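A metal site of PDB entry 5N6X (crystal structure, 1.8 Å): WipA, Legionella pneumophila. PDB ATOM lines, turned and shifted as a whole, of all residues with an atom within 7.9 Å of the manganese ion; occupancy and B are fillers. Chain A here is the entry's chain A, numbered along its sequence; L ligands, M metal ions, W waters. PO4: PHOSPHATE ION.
The manganese ion is bound by OD1 of Asn 191, at 2.2 Å.
The manganese ion is bound by OD2 of Asp 159.
O1 of the ligand binds the manganese ion, 2.2 Å away.
The manganese ion is bound by water W1, 2.2 Å away.
NE2 of His 269 binds the manganese ion.
Water W2 is bound to the manganese ion (2.2 Å).
The backbone carbonyl oxygen (O) of Val 345 lies close to the side-chain amide oxygen (OD1) of Asn 191 (3.3 Å).
N of Asp 159 sits at hydrogen-bond distance from OG of Ser 190 (2.8 Å).
The backbone carbonyl oxygen of Asp 159 is in hydrogen-bond range of the backbone NH of His 11 (3.2 Å).
N of Gly 373 lies within hydrogen-bond range of O of His 269, at 2.9 Å.
The side-chain carboxylate (OD1) of Asp 159 sits at hydrogen-bond distance from the backbone NH (N) of His 192.
ND1 of His 269 is in hydrogen-bond range of O of Leu 157 (2.8 Å).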
ATOM      1  N   HIS A  11      16.587  23.289   5.033  1.00  0.00           N
ATOM      2  CA  HIS A  11      17.266  24.069   6.076  1.00  0.00           C
ATOM      3  C   HIS A  11      16.451  25.295   6.504  1.00  0.00           C
ATOM      4  O   HIS A  11      16.982  26.407   6.625  1.00  0.00           O
ATOM      5  CB  HIS A  11      18.667  24.484   5.627  1.00  0.00           C
ATOM      6  CG  HIS A  11      19.596  23.343   5.431  1.00  0.00           C
ATOM      7  ND1 HIS A  11      19.888  22.824   4.188  1.00  0.00           N
ATOM      8  CD2 HIS A  11      20.289  22.599   6.321  1.00  0.00           C
ATOM      9  CE1 HIS A  11      20.733  21.809   4.328  1.00  0.00           C
ATOM     10  NE2 HIS A  11      20.992  21.662   5.608  1.00  0.00           N
ATOM     11  N   LEU A 157      12.283  15.610   3.448  1.00  0.00           N
ATOM     12  CA  LEU A 157      13.072  14.698   4.277  1.00  0.00           C
ATOM     13  C   LEU A 157      13.549  15.334   5.586  1.00  0.00           C
ATOM     14  O   LEU A 157      14.214  14.668   6.378  1.00  0.00           O
ATOM     15  CB  LEU A 157      14.269  14.151   3.464  1.00  0.00           C
ATOM     16  CG  LEU A 157      13.873  13.311   2.247  1.00  0.00           C
ATOM     17  CD1 LEU A 157      15.096  12.629   1.639  1.00  0.00           C
ATOM     18  CD2 LEU A 157      12.821  12.262   2.590  1.00  0.00           C
ATOM     19  N   GLY A 158      13.185  16.588   5.875  1.00  0.00           N
ATOM     20  CA  GLY A 158      13.356  17.107   7.222  1.00  0.00           C
ATOM     21  C   GLY A 158      14.113  18.417   7.252  1.00  0.00           C
ATOM     22  O   GLY A 158      14.470  18.986   6.222  1.00  0.00           O
ATOM     23  N   ASP A 159      14.348  18.889   8.479  1.00  0.00           N
ATOM     24  CA  ASP A 159      14.918  20.213   8.750  1.00  0.00           C
ATOM     25  C   ASP A 159      14.201  21.328   7.975  1.00  0.00           C
ATOM     26  O   ASP A 159      14.818  22.299   7.519  1.00  0.00           O
ATOM     27  CB  ASP A 159      16.433  20.220   8.507  1.00  0.00           C
ATOM     28  CG  ASP A 159      17.213  19.286   9.479  1.00  0.00           C
ATOM     29  OD1 ASP A 159      16.724  18.805  10.520  1.00  0.00           O
ATOM     30  OD2 ASP A 159      18.380  18.973   9.270  1.00  0.00           O
ATOM     31  N   GLU A 160      12.871  21.177   7.847  1.00  0.00           N
ATOM     32  CA  GLU A 160      12.011  22.157   7.175  1.00  0.00           C
ATOM     33  C   GLU A 160      11.713  23.386   8.028  1.00  0.00           C
ATOM     34  O   GLU A 160      11.291  24.418   7.474  1.00  0.00           O
ATOM     35  CB  GLU A 160      10.667  21.500   6.793  1.00  0.00           C
ATOM     36  CG  GLU A 160       9.777  21.072   7.980  1.00  0.00           C
ATOM     37  CD  GLU A 160      10.287  19.855   8.739  1.00  0.00           C
ATOM     38  OE1 GLU A 160      11.239  19.189   8.261  1.00  0.00           O
ATOM     39  OE2 GLU A 160       9.771  19.541   9.828  1.00  0.00           O
ATOM     40  N   ASP A 163      15.538  26.046  11.571  1.00  0.00           N
ATOM     41  CA  ASP A 163      16.861  25.839  10.984  1.00  0.00           C
ATOM     42  C   ASP A 163      17.412  27.209  10.593  1.00  0.00           C
ATOM     43  O   ASP A 163      16.975  28.242  11.117  1.00  0.00           O
ATOM     44  CB  ASP A 163      16.759  24.791   9.844  1.00  0.00           C
ATOM     45  CG  ASP A 163      18.105  24.143   9.497  1.00  0.00           C
ATOM     46  OD1 ASP A 163      19.099  24.866   9.262  1.00  0.00           O
ATOM     47  OD2 ASP A 163      18.161  22.910   9.418  1.00  0.00           O
ATOM     48  N   ARG A 164      18.361  27.241   9.668  1.00  0.00           N
ATOM     49  CA  ARG A 164      19.167  28.434   9.459  1.00  0.00           C
ATOM     50  C   ARG A 164      18.484  29.520   8.633  1.00  0.00           C
ATOM     51  O   ARG A 164      19.017  30.634   8.557  1.00  0.00           O
ATOM     52  CB  ARG A 164      20.501  28.044   8.823  1.00  0.00           C
ATOM     53  CG  ARG A 164      21.376  27.220   9.743  1.00  0.00           C
ATOM     54  CD  ARG A 164      22.276  26.276   8.952  1.00  0.00           C
ATOM     55  NE  ARG A 164      23.101  25.445   9.832  1.00  0.00           N
ATOM     56  CZ  ARG A 164      22.776  24.225  10.244  1.00  0.00           C
ATOM     57  NH1 ARG A 164      21.642  23.657   9.852  1.00  0.00           N
ATOM     58  NH2 ARG A 164      23.603  23.558  11.039  1.00  0.00           N
ATOM     59  N   LEU A 189      10.220  13.410  10.460  1.00  0.00           N
ATOM     60  CA  LEU A 189      10.707  13.980  11.723  1.00  0.00           C
ATOM     61  C   LEU A 189      12.236  14.109  11.700  1.00  0.00           C
ATOM     62  O   LEU A 189      12.956  13.177  11.311  1.00  0.00           O
ATOM     63  CB  LEU A 189      10.274  13.081  12.888  1.00  0.00           C
ATOM     64  CG  LEU A 189      10.557  13.556  14.305  1.00  0.00           C
ATOM     65  CD1 LEU A 189       9.925  14.937  14.597  1.00  0.00           C
ATOM     66  CD2 LEU A 189      10.082  12.486  15.311  1.00  0.00           C
ATOM     67  N   SER A 190      12.704  15.270  12.125  1.00  0.00           N
ATOM     68  CA  SER A 190      14.107  15.621  11.958  1.00  0.00           C
ATOM     69  C   SER A 190      14.627  16.250  13.240  1.00  0.00           C
ATOM     70  O   SER A 190      13.875  16.510  14.188  1.00  0.00           O
ATOM     71  CB  SER A 190      14.313  16.569  10.774  1.00  0.00           C
ATOM     72  OG  SER A 190      13.578  17.765  10.945  1.00  0.00           O
ATOM     73  N   ASN A 191      15.943  16.526  13.283  1.00  0.00           N
ATOM     74  CA  ASN A 191      16.471  17.102  14.517  1.00  0.00           C
ATOM     75  C   ASN A 191      16.076  18.566  14.648  1.00  0.00           C
ATOM     76  O   ASN A 191      15.809  19.038  15.757  1.00  0.00           O
ATOM     77  CB  ASN A 191      17.992  16.895  14.630  1.00  0.00           C
ATOM     78  CG  ASN A 191      18.788  17.443  13.449  1.00  0.00           C
ATOM     79  OD1 ASN A 191      18.370  17.366  12.306  1.00  0.00           O
ATOM     80  ND2 ASN A 191      19.991  17.954  13.741  1.00  0.00           N
ATOM     81  N   HIS A 192      16.008  19.311  13.531  1.00  0.00           N
ATOM     82  CA  HIS A 192      15.492  20.675  13.607  1.00  0.00           C
ATOM     83  C   HIS A 192      13.975  20.699  13.755  1.00  0.00           C
ATOM     84  O   HIS A 192      13.438  21.521  14.514  1.00  0.00           O
ATOM     85  CB  HIS A 192      15.947  21.485  12.383  1.00  0.00           C
ATOM     86  CG  HIS A 192      17.416  21.776  12.371  1.00  0.00           C
ATOM     87  ND1 HIS A 192      17.945  23.006  12.710  1.00  0.00           N
ATOM     88  CD2 HIS A 192      18.483  20.966  12.111  1.00  0.00           C
ATOM     89  CE1 HIS A 192      19.266  22.958  12.628  1.00  0.00           C
ATOM     90  NE2 HIS A 192      19.620  21.734  12.280  1.00  0.00           N
ATOM     91  N   GLY A 193      13.262  19.807  13.062  1.00  0.00           N
ATOM     92  CA  GLY A 193      11.828  19.703  13.283  1.00  0.00           C
ATOM     93  C   GLY A 193      11.496  19.441  14.747  1.00  0.00           C
ATOM     94  O   GLY A 193      10.541  20.011  15.288  1.00  0.00           O
ATOM     95  N   ILE A 215      20.280  22.700  19.833  1.00  0.00           N
ATOM     96  CA  ILE A 215      20.784  23.426  18.670  1.00  0.00           C
ATOM     97  C   ILE A 215      20.828  24.907  18.999  1.00  0.00           C
ATOM     98  O   ILE A 215      19.867  25.465  19.550  1.00  0.00           O
ATOM     99  CB  ILE A 215      19.892  23.130  17.456  1.00  0.00           C
ATOM    100  CG1 ILE A 215      19.818  21.617  17.203  1.00  0.00           C
ATOM    101  CG2 ILE A 215      20.420  23.843  16.217  1.00  0.00           C
ATOM    102  CD1 ILE A 215      18.957  21.232  16.000  1.00  0.00           C
ATOM    103  N   HIS A 269      15.348  10.853   7.803  1.00  0.00           N
ATOM    104  CA  HIS A 269      15.972  12.176   7.802  1.00  0.00           C
ATOM    105  C   HIS A 269      17.487  12.042   7.751  1.00  0.00           C
ATOM    106  O   HIS A 269      18.138  12.523   6.819  1.00  0.00           O
ATOM    107  CB  HIS A 269      15.554  12.990   9.033  1.00  0.00           C
ATOM    108  CG  HIS A 269      16.297  14.285   9.139  1.00  0.00           C
ATOM    109  ND1 HIS A 269      16.257  15.234   8.146  1.00  0.00           N
ATOM    110  CD2 HIS A 269      17.168  14.746  10.075  1.00  0.00           C
ATOM    111  CE1 HIS A 269      17.050  16.240   8.467  1.00  0.00           C
ATOM    112  NE2 HIS A 269      17.621  15.960   9.628  1.00  0.00           N
ATOM    113  N   ALA A 270      18.049  11.404   8.772  1.00  0.00           N
ATOM    114  CA  ALA A 270      19.461  11.034   8.802  1.00  0.00           C
ATOM    115  C   ALA A 270      19.672   9.729   8.052  1.00  0.00           C
ATOM    116  O   ALA A 270      18.732   8.952   7.866  1.00  0.00           O
ATOM    117  CB  ALA A 270      19.920  10.868  10.251  1.00  0.00           C
ATOM    118  N   LEU A 344      17.756   8.325  14.782  1.00  0.00           N
ATOM    119  CA  LEU A 344      17.105   8.508  13.490  1.00  0.00           C
ATOM    120  C   LEU A 344      17.152   9.941  12.974  1.00  0.00           C
ATOM    121  O   LEU A 344      17.062  10.138  11.762  1.00  0.00           O
ATOM    122  CB  LEU A 344      15.634   8.072  13.541  1.00  0.00           C
ATOM    123  CG  LEU A 344      15.234   6.589  13.687  1.00  0.00           C
ATOM    124  CD1 LEU A 344      13.753   6.412  13.281  1.00  0.00           C
ATOM    125  CD2 LEU A 344      16.107   5.619  12.958  1.00  0.00           C
ATOM    126  N   VAL A 345      17.274  10.948  13.836  1.00  0.00           N
ATOM    127  CA  VAL A 345      17.262  12.335  13.377  1.00  0.00           C
ATOM    128  C   VAL A 345      18.619  13.005  13.469  1.00  0.00           C
ATOM    129  O   VAL A 345      18.780  14.097  12.893  1.00  0.00           O
ATOM    130  CB  VAL A 345      16.209  13.177  14.122  1.00  0.00           C
ATOM    131  CG1 VAL A 345      14.849  12.500  14.073  1.00  0.00           C
ATOM    132  CG2 VAL A 345      16.620  13.450  15.578  1.00  0.00           C
ATOM    133  N   TRP A 346      19.602  12.395  14.165  1.00  0.00           N
ATOM    134  CA  TRP A 346      20.907  13.017  14.368  1.00  0.00           C
ATOM    135  C   TRP A 346      22.080  12.292  13.692  1.00  0.00           C
ATOM    136  O   TRP A 346      23.134  12.904  13.518  1.00  0.00           O
ATOM    137  CB  TRP A 346      21.236  13.121  15.864  1.00  0.00           C
ATOM    138  CG  TRP A 346      20.661  14.350  16.506  1.00  0.00           C
ATOM    139  CD1 TRP A 346      19.518  14.438  17.215  1.00  0.00           C
ATOM    140  CD2 TRP A 346      21.202  15.679  16.441  1.00  0.00           C
ATOM    141  NE1 TRP A 346      19.305  15.737  17.628  1.00  0.00           N
ATOM    142  CE2 TRP A 346      20.331  16.514  17.152  1.00  0.00           C
ATOM    143  CE3 TRP A 346      22.353  16.229  15.849  1.00  0.00           C
ATOM    144  CZ2 TRP A 346      20.554  17.891  17.296  1.00  0.00           C
ATOM    145  CZ3 TRP A 346      22.579  17.597  15.983  1.00  0.00           C
ATOM    146  CH2 TRP A 346      21.684  18.412  16.713  1.00  0.00           C
ATOM    147  N   ASN A 347      21.936  11.005  13.341  1.00  0.00           N
ATOM    148  CA  ASN A 347      23.086  10.245  12.854  1.00  0.00           C
ATOM    149  C   ASN A 347      23.719  10.916  11.631  1.00  0.00           C
ATOM    150  O   ASN A 347      23.030  11.456  10.774  1.00  0.00           O
ATOM    151  CB  ASN A 347      22.684   8.810  12.508  1.00  0.00           C
ATOM    152  CG  ASN A 347      23.884   7.881  12.332  1.00  0.00           C
ATOM    153  OD1 ASN A 347      24.843   7.908  13.125  1.00  0.00           O
ATOM    154  ND2 ASN A 347      23.842   7.040  11.277  1.00  0.00           N
ATOM    155  N   ARG A 348      25.061  10.879  11.587  1.00  0.00           N
ATOM    156  CA  ARG A 348      25.829  11.241  10.403  1.00  0.00           C
ATOM    157  C   ARG A 348      26.693  10.054   9.997  1.00  0.00           C
ATOM    158  O   ARG A 348      27.392   9.482  10.837  1.00  0.00           O
ATOM    159  CB  ARG A 348      26.696  12.466  10.656  1.00  0.00           C
ATOM    160  CG  ARG A 348      25.848  13.724  10.908  1.00  0.00           C
ATOM    161  CD  ARG A 348      26.645  15.003  10.971  1.00  0.00           C
ATOM    162  NE  ARG A 348      25.754  16.093  11.383  1.00  0.00           N
ATOM    163  CZ  ARG A 348      26.148  17.192  12.002  1.00  0.00           C
ATOM    164  NH1 ARG A 348      27.432  17.377  12.288  1.00  0.00           N
ATOM    165  NH2 ARG A 348      25.252  18.109  12.358  1.00  0.00           N
ATOM    166  N   GLY A 373      17.984  12.535   3.948  1.00  0.00           N
ATOM    167  CA  GLY A 373      18.334  13.921   3.752  1.00  0.00           C
ATOM    168  C   GLY A 373      19.832  14.134   3.701  1.00  0.00           C
ATOM    169  O   GLY A 373      20.619  13.253   4.025  1.00  0.00           O
ATOM    170  N   HIS A 374      20.204  15.358   3.313  1.00  0.00           N
ATOM    171  CA  HIS A 374      21.603  15.735   3.093  1.00  0.00           C
ATOM    172  C   HIS A 374      22.500  15.212   4.217  1.00  0.00           C
ATOM    173  O   HIS A 374      22.171  15.327   5.400  1.00  0.00           O
ATOM    174  CB  HIS A 374      21.729  17.263   3.011  1.00  0.00           C
ATOM    175  CG  HIS A 374      21.305  17.955   4.258  1.00  0.00           C
ATOM    176  ND1 HIS A 374      19.983  18.179   4.585  1.00  0.00           N
ATOM    177  CD2 HIS A 374      22.022  18.435   5.305  1.00  0.00           C
ATOM    178  CE1 HIS A 374      19.902  18.776   5.761  1.00  0.00           C
ATOM    179  NE2 HIS A 374      21.134  18.946   6.216  1.00  0.00           N
HETATM  180  P   PO4 L   1      21.911  19.606  10.545  1.00  0.00           P
HETATM  181  O1  PO4 L   1      20.929  18.543  10.986  1.00  0.00           O
HETATM  182  O2  PO4 L   1      23.249  18.943  10.267  1.00  0.00           O
HETATM  183  O3  PO4 L   1      21.461  20.269   9.269  1.00  0.00           O
HETATM  184  O4  PO4 L   1      22.073  20.688  11.600  1.00  0.00           O
HETATM  185 MN    MN M   1      19.257  17.291  10.329  1.00  0.00          MN
HETATM  186  O   HOH W   1      20.451  16.823   8.518  1.00  0.00           O
HETATM  187  O   HOH W   2      20.357  15.515  11.162  1.00  0.00           O
